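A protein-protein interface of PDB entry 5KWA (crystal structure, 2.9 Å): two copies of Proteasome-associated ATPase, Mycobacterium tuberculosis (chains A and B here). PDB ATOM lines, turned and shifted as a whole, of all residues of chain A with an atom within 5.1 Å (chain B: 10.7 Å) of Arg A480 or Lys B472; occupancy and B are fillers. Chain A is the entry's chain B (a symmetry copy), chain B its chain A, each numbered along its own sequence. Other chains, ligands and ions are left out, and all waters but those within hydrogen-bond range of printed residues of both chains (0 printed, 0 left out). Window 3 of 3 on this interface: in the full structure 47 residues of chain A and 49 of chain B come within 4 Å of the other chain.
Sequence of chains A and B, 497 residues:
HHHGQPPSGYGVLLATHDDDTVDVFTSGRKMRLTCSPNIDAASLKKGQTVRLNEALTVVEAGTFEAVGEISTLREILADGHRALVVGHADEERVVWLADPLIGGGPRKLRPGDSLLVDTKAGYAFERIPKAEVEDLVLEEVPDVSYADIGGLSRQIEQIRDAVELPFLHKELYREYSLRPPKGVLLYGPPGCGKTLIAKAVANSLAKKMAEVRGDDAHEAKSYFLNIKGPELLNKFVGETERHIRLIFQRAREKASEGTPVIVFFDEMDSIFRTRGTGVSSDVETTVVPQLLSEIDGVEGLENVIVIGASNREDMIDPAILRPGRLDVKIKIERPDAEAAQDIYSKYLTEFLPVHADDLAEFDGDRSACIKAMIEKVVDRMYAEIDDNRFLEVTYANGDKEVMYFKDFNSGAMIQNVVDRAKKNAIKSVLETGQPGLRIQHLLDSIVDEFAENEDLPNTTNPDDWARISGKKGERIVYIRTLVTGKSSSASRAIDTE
No position is printed for both chains. Of the 13 pairs that touch across the chains among the printed residues, none has its exchanged pair printed and touching as well.
OH of Tyr A478 touches N of Gly B470, 3.8 Å away. Tyr A478 touches Gly B473. Tyr A478 touches Arg B475 (CD1 to CG, 3.4 Å). Lys B471 touches Arg A480 (O to NH1, 3.997 Å). Arg A480 touches Lys B472 (NH1 to C, 3.9 Å). Arg A492 touches Ala B466 (CA to O, 3.6 Å). CD of Arg A492 touches N of Arg B467, at 3.7 Å. Ala A493 touches Ser B469.
The backbone carbonyl oxygen of Arg B475 is in hydrogen-bond range of the backbone NH of Ala B396. The side-chain amino group (NZ) of Lys B472 is in salt-bridge range of the side-chain carboxylate (OD2) of Asp B399 (3.3 Å). NH2 of Arg B467 lies within salt-bridge range of OD1 of Asp B464. The backbone carbonyl oxygen of Glu B474 sits at hydrogen-bond distance from the side-chain hydroxyl of Ser B469, at 2.6 Å. OE2 of Glu A392 is in salt-bridge range of NH2 of Arg A480 (2.8 Å). The backbone NH (N) of Thr A481 sits at hydrogen-bond distance from the backbone carbonyl oxygen (O) of Arg A492.
O of Ala B466 lies within hydrogen-bond range of N of Ala A493, at 3.3 Å. The side-chain hydroxyl of Tyr A478 sits at hydrogen-bond distance from the backbone carbonyl oxygen of Ser B469 (2.7 Å). The guanidinium group (NH1) of Arg A480 sits close to the backbone carbonyl oxygen (O) of Gly B470 (3.1 Å). The backbone NH (N) of Glu B474 is in hydrogen-bond range of the side-chain hydroxyl (OH) of Tyr A478 (3.4 Å). The backbone NH (N) of Gly B473 sits close to the guanidinium group (NH1) of Arg A480 (3.4 Å).
Hydrophobic or aromatic side chains of chain B that line the printed part of chain A: Ala B466. Along chain B the printed residues that touch a printed residue of chain A span positions 466 to 475. Among the printed residues, 13 pairs touch across the chains. Among the printed residues, no Asp or Glu carboxylate lies within 4 Å of a Lys or Arg side-chain nitrogen of the other chain.
Of the printed residues of chain B, Arg A480 touches Gly B470 (3.0 Å), Lys B471 (3.997 Å), Lys B472 (3.9 Å) and Gly B473 (3.2 Å). Lys B472 touches just one residue of chain A: Arg A480 (3.9 Å). Glu A392 touches none of the printed residues of chain B. No residue of chain B comes within 4 Å of Ile A479. No residue of chain B comes within 4 Å of Thr A481. Ala A493 touches two residues of chain B. Printed residues of chain A within 4 Å of Gly B470: Tyr A478 (3.8 Å) and Arg A480 (3.0 Å). Of the printed residues of chain A, Arg B467 touches Arg A492 (3.7 Å). Printed residues of chain A within 4 Å of Glu B474: Tyr A478 (3.4 Å). Printed residues of chain A within 4 Å of Arg B475: Tyr A478. Asp B464 touches none of the printed residues of chain A. Asp B399 touches none of the printed residues of chain A. The nearest printed residue of chain B that does not touch Arg A480 is Ser B469 (4.8 Å). The nearest printed residue of chain A that does not touch Gly B473 is Glu A392 (5.6 Å).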
ATOM      1  N   PHE A 390       9.340  -7.518   3.298  1.00  0.00           N
ATOM      2  CA  PHE A 390       9.808  -6.866   4.517  1.00  0.00           C
ATOM      3  C   PHE A 390       8.734  -6.005   5.172  1.00  0.00           C
ATOM      4  O   PHE A 390       8.475  -6.150   6.365  1.00  0.00           O
ATOM      5  CB  PHE A 390      11.052  -6.027   4.194  1.00  0.00           C
ATOM      6  CG  PHE A 390      11.723  -5.422   5.405  1.00  0.00           C
ATOM      7  CD1 PHE A 390      12.093  -6.212   6.491  1.00  0.00           C
ATOM      8  CD2 PHE A 390      12.005  -4.057   5.448  1.00  0.00           C
ATOM      9  CE1 PHE A 390      12.704  -5.647   7.599  1.00  0.00           C
ATOM     10  CE2 PHE A 390      12.614  -3.487   6.554  1.00  0.00           C
ATOM     11  CZ  PHE A 390      12.967  -4.282   7.629  1.00  0.00           C
ATOM     12  N   LEU A 391       8.141  -5.099   4.393  1.00  0.00           N
ATOM     13  CA  LEU A 391       7.090  -4.193   4.854  1.00  0.00           C
ATOM     14  C   LEU A 391       5.869  -4.232   3.956  1.00  0.00           C
ATOM     15  O   LEU A 391       5.938  -4.674   2.811  1.00  0.00           O
ATOM     16  CB  LEU A 391       7.610  -2.756   4.886  1.00  0.00           C
ATOM     17  CG  LEU A 391       8.081  -2.227   6.239  1.00  0.00           C
ATOM     18  CD1 LEU A 391       9.138  -3.120   6.879  1.00  0.00           C
ATOM     19  CD2 LEU A 391       8.600  -0.815   6.049  1.00  0.00           C
ATOM     20  N   GLU A 392       4.757  -3.754   4.500  1.00  0.00           N
ATOM     21  CA  GLU A 392       3.560  -3.449   3.729  1.00  0.00           C
ATOM     22  C   GLU A 392       3.107  -2.056   4.132  1.00  0.00           C
ATOM     23  O   GLU A 392       2.811  -1.807   5.306  1.00  0.00           O
ATOM     24  CB  GLU A 392       2.439  -4.451   3.991  1.00  0.00           C
ATOM     25  CG  GLU A 392       1.252  -4.308   3.034  1.00  0.00           C
ATOM     26  CD  GLU A 392      -0.094  -4.294   3.747  1.00  0.00           C
ATOM     27  OE1 GLU A 392      -0.292  -3.441   4.646  1.00  0.00           O
ATOM     28  OE2 GLU A 392      -0.954  -5.138   3.405  1.00  0.00           O
ATOM     29  N   TYR A 478      -0.439   3.645   7.499  1.00  0.00           N
ATOM     30  CA  TYR A 478      -0.243   2.393   8.252  1.00  0.00           C
ATOM     31  C   TYR A 478       0.911   1.575   7.657  1.00  0.00           C
ATOM     32  O   TYR A 478       0.951   1.348   6.449  1.00  0.00           O
ATOM     33  CB  TYR A 478      -1.550   1.577   8.272  1.00  0.00           C
ATOM     34  CG  TYR A 478      -1.470   0.226   8.972  1.00  0.00           C
ATOM     35  CD1 TYR A 478      -1.441   0.141  10.365  1.00  0.00           C
ATOM     36  CD2 TYR A 478      -1.440  -0.970   8.238  1.00  0.00           C
ATOM     37  CE1 TYR A 478      -1.373  -1.088  11.012  1.00  0.00           C
ATOM     38  CE2 TYR A 478      -1.373  -2.205   8.876  1.00  0.00           C
ATOM     39  CZ  TYR A 478      -1.342  -2.259  10.263  1.00  0.00           C
ATOM     40  OH  TYR A 478      -1.277  -3.474  10.907  1.00  0.00           O
ATOM     41  N   ILE A 479       1.847   1.154   8.514  1.00  0.00           N
ATOM     42  CA  ILE A 479       2.988   0.310   8.122  1.00  0.00           C
ATOM     43  C   ILE A 479       2.892  -1.017   8.877  1.00  0.00           C
ATOM     44  O   ILE A 479       2.437  -1.058  10.018  1.00  0.00           O
ATOM     45  CB  ILE A 479       4.353   0.988   8.431  1.00  0.00           C
ATOM     46  CG1 ILE A 479       4.523   2.279   7.614  1.00  0.00           C
ATOM     47  CG2 ILE A 479       5.522   0.047   8.136  1.00  0.00           C
ATOM     48  CD1 ILE A 479       5.586   3.220   8.152  1.00  0.00           C
ATOM     49  N   ARG A 480       3.327  -2.091   8.225  1.00  0.00           N
ATOM     50  CA  ARG A 480       3.330  -3.427   8.812  1.00  0.00           C
ATOM     51  C   ARG A 480       4.513  -4.249   8.277  1.00  0.00           C
ATOM     52  O   ARG A 480       4.762  -4.251   7.072  1.00  0.00           O
ATOM     53  CB  ARG A 480       1.994  -4.108   8.495  1.00  0.00           C
ATOM     54  CG  ARG A 480       2.007  -5.621   8.590  1.00  0.00           C
ATOM     55  CD  ARG A 480       0.623  -6.216   8.448  1.00  0.00           C
ATOM     56  NE  ARG A 480       0.192  -6.334   7.056  1.00  0.00           N
ATOM     57  CZ  ARG A 480      -0.782  -7.139   6.622  1.00  0.00           C
ATOM     58  NH1 ARG A 480      -1.467  -7.926   7.454  1.00  0.00           N
ATOM     59  NH2 ARG A 480      -1.081  -7.162   5.328  1.00  0.00           N
ATOM     60  N   THR A 481       5.233  -4.937   9.165  1.00  0.00           N
ATOM     61  CA  THR A 481       6.299  -5.869   8.759  1.00  0.00           C
ATOM     62  C   THR A 481       5.700  -7.232   8.396  1.00  0.00           C
ATOM     63  O   THR A 481       4.565  -7.540   8.787  1.00  0.00           O
ATOM     64  CB  THR A 481       7.376  -6.072   9.853  1.00  0.00           C
ATOM     65  OG1 THR A 481       6.807  -6.743  10.980  1.00  0.00           O
ATOM     66  CG2 THR A 481       7.990  -4.742  10.303  1.00  0.00           C
ATOM     67  N   LEU A 482       6.474  -8.043   7.670  1.00  0.00           N
ATOM     68  CA  LEU A 482       5.991  -9.316   7.104  1.00  0.00           C
ATOM     69  C   LEU A 482       6.995 -10.461   7.292  1.00  0.00           C
ATOM     70  O   LEU A 482       7.933 -10.629   6.512  1.00  0.00           O
ATOM     71  CB  LEU A 482       5.653  -9.129   5.615  1.00  0.00           C
ATOM     72  CG  LEU A 482       4.618  -8.054   5.242  1.00  0.00           C
ATOM     73  CD1 LEU A 482       4.572  -7.884   3.730  1.00  0.00           C
ATOM     74  CD2 LEU A 482       3.229  -8.372   5.782  1.00  0.00           C
ATOM     75  N   ARG A 492       4.436  -7.614  12.479  1.00  0.00           N
ATOM     76  CA  ARG A 492       4.312  -6.496  13.452  1.00  0.00           C
ATOM     77  C   ARG A 492       3.982  -5.171  12.749  1.00  0.00           C
ATOM     78  O   ARG A 492       4.269  -5.010  11.567  1.00  0.00           O
ATOM     79  CB  ARG A 492       5.613  -6.294  14.244  1.00  0.00           C
ATOM     80  CG  ARG A 492       6.159  -7.513  14.975  1.00  0.00           C
ATOM     81  CD  ARG A 492       5.374  -7.836  16.235  1.00  0.00           C
ATOM     82  NE  ARG A 492       5.938  -8.988  16.946  1.00  0.00           N
ATOM     83  CZ  ARG A 492       5.809 -10.268  16.578  1.00  0.00           C
ATOM     84  NH1 ARG A 492       5.130 -10.616  15.486  1.00  0.00           N
ATOM     85  NH2 ARG A 492       6.373 -11.227  17.314  1.00  0.00           N
ATOM     86  N   ALA A 493       3.404  -4.225  13.490  1.00  0.00           N
ATOM     87  CA  ALA A 493       3.065  -2.884  12.976  1.00  0.00           C
ATOM     88  C   ALA A 493       4.036  -1.825  13.497  1.00  0.00           C
ATOM     89  O   ALA A 493       4.714  -2.036  14.506  1.00  0.00           O
ATOM     90  CB  ALA A 493       1.637  -2.517  13.350  1.00  0.00           C
ATOM     91  N   ILE A 494       4.100  -0.698  12.784  1.00  0.00           N
ATOM     92  CA  ILE A 494       4.968   0.443  13.138  1.00  0.00           C
ATOM     93  C   ILE A 494       4.192   1.753  12.945  1.00  0.00           C
ATOM     94  O   ILE A 494       3.478   1.915  11.952  1.00  0.00           O
ATOM     95  CB  ILE A 494       6.268   0.512  12.283  1.00  0.00           C
ATOM     96  CG1 ILE A 494       6.858  -0.885  12.011  1.00  0.00           C
ATOM     97  CG2 ILE A 494       7.305   1.402  12.969  1.00  0.00           C
ATOM     98  CD1 ILE A 494       8.018  -0.893  11.037  1.00  0.00           C
ATOM     99  N   VAL B 393     -10.294  -6.894  20.881  1.00  0.00           N
ATOM    100  CA  VAL B 393      -9.610  -5.894  20.071  1.00  0.00           C
ATOM    101  C   VAL B 393     -10.533  -5.503  18.928  1.00  0.00           C
ATOM    102  O   VAL B 393     -10.840  -6.335  18.081  1.00  0.00           O
ATOM    103  CB  VAL B 393      -8.280  -6.452  19.518  1.00  0.00           C
ATOM    104  CG1 VAL B 393      -7.748  -5.600  18.370  1.00  0.00           C
ATOM    105  CG2 VAL B 393      -7.251  -6.544  20.638  1.00  0.00           C
ATOM    106  N   THR B 394     -10.960  -4.239  18.924  1.00  0.00           N
ATOM    107  CA  THR B 394     -11.741  -3.652  17.835  1.00  0.00           C
ATOM    108  C   THR B 394     -10.790  -2.938  16.882  1.00  0.00           C
ATOM    109  O   THR B 394      -9.909  -2.205  17.327  1.00  0.00           O
ATOM    110  CB  THR B 394     -12.773  -2.641  18.374  1.00  0.00           C
ATOM    111  OG1 THR B 394     -13.687  -3.310  19.252  1.00  0.00           O
ATOM    112  CG2 THR B 394     -13.549  -1.976  17.241  1.00  0.00           C
ATOM    113  N   TYR B 395     -10.988  -3.139  15.580  1.00  0.00           N
ATOM    114  CA  TYR B 395     -10.107  -2.582  14.543  1.00  0.00           C
ATOM    115  C   TYR B 395     -10.687  -1.321  13.879  1.00  0.00           C
ATOM    116  O   TYR B 395     -11.854  -0.967  14.093  1.00  0.00           O
ATOM    117  CB  TYR B 395      -9.797  -3.658  13.487  1.00  0.00           C
ATOM    118  CG  TYR B 395      -8.978  -4.813  14.026  1.00  0.00           C
ATOM    119  CD1 TYR B 395      -7.647  -4.636  14.391  1.00  0.00           C
ATOM    120  CD2 TYR B 395      -9.530  -6.078  14.169  1.00  0.00           C
ATOM    121  CE1 TYR B 395      -6.890  -5.685  14.887  1.00  0.00           C
ATOM    122  CE2 TYR B 395      -8.781  -7.136  14.666  1.00  0.00           C
ATOM    123  CZ  TYR B 395      -7.463  -6.935  15.024  1.00  0.00           C
ATOM    124  OH  TYR B 395      -6.719  -7.983  15.517  1.00  0.00           O
ATOM    125  N   ALA B 396      -9.856  -0.661  13.070  1.00  0.00           N
ATOM    126  CA  ALA B 396     -10.241   0.559  12.338  1.00  0.00           C
ATOM    127  C   ALA B 396     -11.274   0.349  11.222  1.00  0.00           C
ATOM    128  O   ALA B 396     -11.841   1.325  10.735  1.00  0.00           O
ATOM    129  CB  ALA B 396      -9.002   1.246  11.770  1.00  0.00           C
ATOM    130  N   ASN B 397     -11.489  -0.901  10.802  1.00  0.00           N
ATOM    131  CA  ASN B 397     -12.524  -1.245   9.813  1.00  0.00           C
ATOM    132  C   ASN B 397     -13.816  -1.796  10.440  1.00  0.00           C
ATOM    133  O   ASN B 397     -14.734  -2.171   9.710  1.00  0.00           O
ATOM    134  CB  ASN B 397     -11.966  -2.237   8.773  1.00  0.00           C
ATOM    135  CG  ASN B 397     -11.594  -3.591   9.370  1.00  0.00           C
ATOM    136  OD1 ASN B 397     -11.411  -3.724  10.581  1.00  0.00           O
ATOM    137  ND2 ASN B 397     -11.466  -4.598   8.513  1.00  0.00           N
ATOM    138  N   GLY B 398     -13.876  -1.847  11.775  1.00  0.00           N
ATOM    139  CA  GLY B 398     -15.061  -2.310  12.508  1.00  0.00           C
ATOM    140  C   GLY B 398     -15.005  -3.744  13.016  1.00  0.00           C
ATOM    141  O   GLY B 398     -15.801  -4.121  13.881  1.00  0.00           O
ATOM    142  N   ASP B 399     -14.083  -4.548  12.484  1.00  0.00           N
ATOM    143  CA  ASP B 399     -13.937  -5.944  12.911  1.00  0.00           C
ATOM    144  C   ASP B 399     -13.447  -6.056  14.352  1.00  0.00           C
ATOM    145  O   ASP B 399     -12.754  -5.174  14.859  1.00  0.00           O
ATOM    146  CB  ASP B 399     -12.965  -6.709  11.997  1.00  0.00           C
ATOM    147  CG  ASP B 399     -13.531  -6.972  10.610  1.00  0.00           C
ATOM    148  OD1 ASP B 399     -14.695  -6.594  10.329  1.00  0.00           O
ATOM    149  OD2 ASP B 399     -12.792  -7.570   9.797  1.00  0.00           O
ATOM    150  N   LYS B 400     -13.820  -7.159  14.992  1.00  0.00           N
ATOM    151  CA  LYS B 400     -13.442  -7.443  16.368  1.00  0.00           C
ATOM    152  C   LYS B 400     -12.885  -8.858  16.478  1.00  0.00           C
ATOM    153  O   LYS B 400     -13.340  -9.777  15.794  1.00  0.00           O
ATOM    154  CB  LYS B 400     -14.639  -7.277  17.303  1.00  0.00           C
ATOM    155  CG  LYS B 400     -15.341  -5.937  17.169  1.00  0.00           C
ATOM    156  CD  LYS B 400     -16.395  -5.744  18.245  1.00  0.00           C
ATOM    157  CE  LYS B 400     -17.370  -4.633  17.873  1.00  0.00           C
ATOM    158  NZ  LYS B 400     -18.518  -4.584  18.814  1.00  0.00           N
ATOM    159  N   GLU B 401     -11.887  -9.013  17.341  1.00  0.00           N
ATOM    160  CA  GLU B 401     -11.269 -10.300  17.609  1.00  0.00           C
ATOM    161  C   GLU B 401     -11.161 -10.465  19.116  1.00  0.00           C
ATOM    162  O   GLU B 401     -10.789  -9.523  19.817  1.00  0.00           O
ATOM    163  CB  GLU B 401      -9.881 -10.354  16.971  1.00  0.00           C
ATOM    164  CG  GLU B 401      -9.088 -11.623  17.285  1.00  0.00           C
ATOM    165  CD  GLU B 401      -7.715 -11.660  16.642  1.00  0.00           C
ATOM    166  OE1 GLU B 401      -7.272 -10.629  16.088  1.00  0.00           O
ATOM    167  OE2 GLU B 401      -7.074 -12.731  16.710  1.00  0.00           O
ATOM    168  N   VAL B 402     -11.488 -11.661  19.599  1.00  0.00           N
ATOM    169  CA  VAL B 402     -11.339 -12.009  21.007  1.00  0.00           C
ATOM    170  C   VAL B 402      -9.957 -12.608  21.206  1.00  0.00           C
ATOM    171  O   VAL B 402      -9.620 -13.586  20.556  1.00  0.00           O
ATOM    172  CB  VAL B 402     -12.386 -13.055  21.447  1.00  0.00           C
ATOM    173  CG1 VAL B 402     -12.203 -13.427  22.921  1.00  0.00           C
ATOM    174  CG2 VAL B 402     -13.798 -12.545  21.182  1.00  0.00           C
ATOM    175  N   MET B 403      -9.171 -12.025  22.106  1.00  0.00           N
ATOM    176  CA  MET B 403      -7.890 -12.598  22.505  1.00  0.00           C
ATOM    177  C   MET B 403      -8.090 -13.433  23.761  1.00  0.00           C
ATOM    178  O   MET B 403      -8.822 -13.020  24.656  1.00  0.00           O
ATOM    179  CB  MET B 403      -6.892 -11.491  22.791  1.00  0.00           C
ATOM    180  CG  MET B 403      -6.786 -10.427  21.705  1.00  0.00           C
ATOM    181  SD  MET B 403      -6.458 -11.100  20.068  1.00  0.00           S
ATOM    182  CE  MET B 403      -4.880 -11.879  20.352  1.00  0.00           C
ATOM    183  N   ASP B 464       2.601  -6.739  21.780  1.00  0.00           N
ATOM    184  CA  ASP B 464       1.383  -7.534  21.546  1.00  0.00           C
ATOM    185  C   ASP B 464       0.453  -6.844  20.537  1.00  0.00           C
ATOM    186  O   ASP B 464      -0.086  -7.491  19.637  1.00  0.00           O
ATOM    187  CB  ASP B 464       0.635  -7.798  22.865  1.00  0.00           C
ATOM    188  CG  ASP B 464       1.520  -8.429  23.934  1.00  0.00           C
ATOM    189  OD1 ASP B 464       2.215  -9.425  23.631  1.00  0.00           O
ATOM    190  OD2 ASP B 464       1.519  -7.924  25.076  1.00  0.00           O
ATOM    191  N   TRP B 465       0.293  -5.530  20.681  1.00  0.00           N
ATOM    192  CA  TRP B 465      -0.584  -4.762  19.799  1.00  0.00           C
ATOM    193  C   TRP B 465       0.042  -4.665  18.430  1.00  0.00           C
ATOM    194  O   TRP B 465      -0.657  -4.745  17.421  1.00  0.00           O
ATOM    195  CB  TRP B 465      -0.879  -3.359  20.343  1.00  0.00           C
ATOM    196  CG  TRP B 465      -1.196  -3.343  21.789  1.00  0.00           C
ATOM    197  CD1 TRP B 465      -0.622  -2.555  22.738  1.00  0.00           C
ATOM    198  CD2 TRP B 465      -2.125  -4.187  22.470  1.00  0.00           C
ATOM    199  NE1 TRP B 465      -1.149  -2.837  23.970  1.00  0.00           N
ATOM    200  CE2 TRP B 465      -2.072  -3.838  23.836  1.00  0.00           C
ATOM    201  CE3 TRP B 465      -3.004  -5.202  22.061  1.00  0.00           C
ATOM    202  CZ2 TRP B 465      -2.856  -4.458  24.795  1.00  0.00           C
ATOM    203  CZ3 TRP B 465      -3.783  -5.824  23.015  1.00  0.00           C
ATOM    204  CH2 TRP B 465      -3.702  -5.444  24.372  1.00  0.00           C
ATOM    205  N   ALA B 466       1.359  -4.495  18.399  1.00  0.00           N
ATOM    206  CA  ALA B 466       2.098  -4.629  17.164  1.00  0.00           C
ATOM    207  C   ALA B 466       1.759  -5.967  16.502  1.00  0.00           C
ATOM    208  O   ALA B 466       1.315  -5.977  15.356  1.00  0.00           O
ATOM    209  CB  ALA B 466       3.590  -4.517  17.424  1.00  0.00           C
ATOM    210  N   ARG B 467       1.913  -7.072  17.241  1.00  0.00           N
ATOM    211  CA  ARG B 467       1.656  -8.435  16.718  1.00  0.00           C
ATOM    212  C   ARG B 467       0.218  -8.639  16.247  1.00  0.00           C
ATOM    213  O   ARG B 467      -0.010  -9.222  15.179  1.00  0.00           O
ATOM    214  CB  ARG B 467       2.015  -9.521  17.759  1.00  0.00           C
ATOM    215  CG  ARG B 467       1.568 -10.941  17.389  1.00  0.00           C
ATOM    216  CD  ARG B 467       2.084 -12.011  18.342  1.00  0.00           C
ATOM    217  NE  ARG B 467       1.448 -11.957  19.666  1.00  0.00           N
ATOM    218  CZ  ARG B 467       1.951 -11.374  20.763  1.00  0.00           C
ATOM    219  NH1 ARG B 467       3.135 -10.751  20.759  1.00  0.00           N
ATOM    220  NH2 ARG B 467       1.251 -11.414  21.897  1.00  0.00           N
ATOM    221  N   ILE B 468      -0.734  -8.178  17.054  1.00  0.00           N
ATOM    222  CA  ILE B 468      -2.154  -8.382  16.770  1.00  0.00           C
ATOM    223  C   ILE B 468      -2.599  -7.467  15.624  1.00  0.00           C
ATOM    224  O   ILE B 468      -3.276  -7.928  14.702  1.00  0.00           O
ATOM    225  CB  ILE B 468      -3.017  -8.194  18.040  1.00  0.00           C
ATOM    226  CG1 ILE B 468      -2.655  -9.259  19.088  1.00  0.00           C
ATOM    227  CG2 ILE B 468      -4.504  -8.295  17.713  1.00  0.00           C
ATOM    228  CD1 ILE B 468      -2.982  -8.852  20.508  1.00  0.00           C
ATOM    229  N   SER B 469      -2.210  -6.190  15.684  1.00  0.00           N
ATOM    230  CA  SER B 469      -2.417  -5.246  14.570  1.00  0.00           C
ATOM    231  C   SER B 469      -1.714  -5.715  13.295  1.00  0.00           C
ATOM    232  O   SER B 469      -2.266  -5.605  12.200  1.00  0.00           O
ATOM    233  CB  SER B 469      -1.913  -3.841  14.930  1.00  0.00           C
ATOM    234  OG  SER B 469      -2.155  -2.910  13.884  1.00  0.00           O
ATOM    235  N   GLY B 470      -0.494  -6.223  13.456  1.00  0.00           N
ATOM    236  CA  GLY B 470       0.279  -6.785  12.362  1.00  0.00           C
ATOM    237  C   GLY B 470      -0.456  -7.920  11.686  1.00  0.00           C
ATOM    238  O   GLY B 470      -0.866  -7.794  10.538  1.00  0.00           O
ATOM    239  N   LYS B 471      -0.674  -9.010  12.412  1.00  0.00           N
ATOM    240  CA  LYS B 471      -1.315 -10.207  11.835  1.00  0.00           C
ATOM    241  C   LYS B 471      -2.656  -9.908  11.129  1.00  0.00           C
ATOM    242  O   LYS B 471      -2.963 -10.516  10.106  1.00  0.00           O
ATOM    243  CB  LYS B 471      -1.505 -11.291  12.907  1.00  0.00           C
ATOM    244  CG  LYS B 471      -1.791 -12.689  12.358  1.00  0.00           C
ATOM    245  CD  LYS B 471      -2.560 -13.548  13.360  1.00  0.00           C
ATOM    246  CE  LYS B 471      -3.291 -14.708  12.689  1.00  0.00           C
ATOM    247  NZ  LYS B 471      -4.356 -15.281  13.562  1.00  0.00           N
ATOM    248  N   LYS B 472      -3.432  -8.970  11.672  1.00  0.00           N
ATOM    249  CA  LYS B 472      -4.693  -8.533  11.057  1.00  0.00           C
ATOM    250  C   LYS B 472      -4.472  -7.587   9.874  1.00  0.00           C
ATOM    251  O   LYS B 472      -5.223  -7.629   8.900  1.00  0.00           O
ATOM    252  CB  LYS B 472      -5.580  -7.836  12.099  1.00  0.00           C
ATOM    253  CG  LYS B 472      -6.955  -7.393  11.603  1.00  0.00           C
ATOM    254  CD  LYS B 472      -7.858  -8.579  11.306  1.00  0.00           C
ATOM    255  CE  LYS B 472      -9.285  -8.139  11.033  1.00  0.00           C
ATOM    256  NZ  LYS B 472     -10.106  -9.264  10.521  1.00  0.00           N
ATOM    257  N   GLY B 473      -3.476  -6.712   9.976  1.00  0.00           N
ATOM    258  CA  GLY B 473      -3.233  -5.684   8.963  1.00  0.00           C
ATOM    259  C   GLY B 473      -4.223  -4.539   9.067  1.00  0.00           C
ATOM    260  O   GLY B 473      -4.647  -3.985   8.054  1.00  0.00           O
ATOM    261  N   GLU B 474      -4.586  -4.195  10.302  1.00  0.00           N
ATOM    262  CA  GLU B 474      -5.502  -3.093  10.602  1.00  0.00           C
ATOM    263  C   GLU B 474      -5.050  -2.405  11.889  1.00  0.00           C
ATOM    264  O   GLU B 474      -4.512  -3.053  12.789  1.00  0.00           O
ATOM    265  CB  GLU B 474      -6.930  -3.621  10.785  1.00  0.00           C
ATOM    266  CG  GLU B 474      -7.683  -3.926   9.496  1.00  0.00           C
ATOM    267  CD  GLU B 474      -8.144  -2.688   8.745  1.00  0.00           C
ATOM    268  OE1 GLU B 474      -8.350  -1.614   9.360  1.00  0.00           O
ATOM    269  OE2 GLU B 474      -8.319  -2.797   7.517  1.00  0.00           O
ATOM    270  N   ARG B 475      -5.278  -1.100  11.978  1.00  0.00           N
ATOM    271  CA  ARG B 475      -4.971  -0.348  13.191  1.00  0.00           C
ATOM    272  C   ARG B 475      -5.975  -0.704  14.279  1.00  0.00           C
ATOM    273  O   ARG B 475      -7.158  -0.901  14.004  1.00  0.00           O
ATOM    274  CB  ARG B 475      -5.032   1.157  12.934  1.00  0.00           C
ATOM    275  CG  ARG B 475      -4.003   1.681  11.942  1.00  0.00           C
ATOM    276  CD  ARG B 475      -4.310   3.116  11.547  1.00  0.00           C
ATOM    277  NE  ARG B 475      -4.433   3.974  12.726  1.00  0.00           N
ATOM    278  CZ  ARG B 475      -4.881   5.230  12.718  1.00  0.00           C
ATOM    279  NH1 ARG B 475      -5.252   5.828  11.585  1.00  0.00           N
ATOM    280  NH2 ARG B 475      -4.949   5.903  13.865  1.00  0.00           N
ATOM    281  N   ILE B 476      -5.498  -0.785  15.512  1.00  0.00           N
ATOM    282  CA  ILE B 476      -6.357  -1.071  16.647  1.00  0.00           C
ATOM    283  C   ILE B 476      -6.879   0.264  17.177  1.00  0.00           C
ATOM    284  O   ILE B 476      -6.094   1.140  17.529  1.00  0.00           O
ATOM    285  CB  ILE B 476      -5.608  -1.888  17.723  1.00  0.00           C
ATOM    286  CG1 ILE B 476      -5.273  -3.277  17.155  1.00  0.00           C
ATOM    287  CG2 ILE B 476      -6.439  -2.007  19.002  1.00  0.00           C
ATOM    288  CD1 ILE B 476      -4.326  -4.103  17.996  1.00  0.00           C
ATOM    289  N   VAL B 477      -8.205   0.403  17.212  1.00  0.00           N
ATOM    290  CA  VAL B 477      -8.879   1.639  17.660  1.00  0.00           C
ATOM    291  C   VAL B 477      -9.490   1.575  19.064  1.00  0.00           C
ATOM    292  O   VAL B 477      -9.583   2.609  19.722  1.00  0.00           O
ATOM    293  CB  VAL B 477      -9.972   2.103  16.663  1.00  0.00           C
ATOM    294  CG1 VAL B 477      -9.385   2.228  15.266  1.00  0.00           C
ATOM    295  CG2 VAL B 477     -11.191   1.183  16.675  1.00  0.00           C
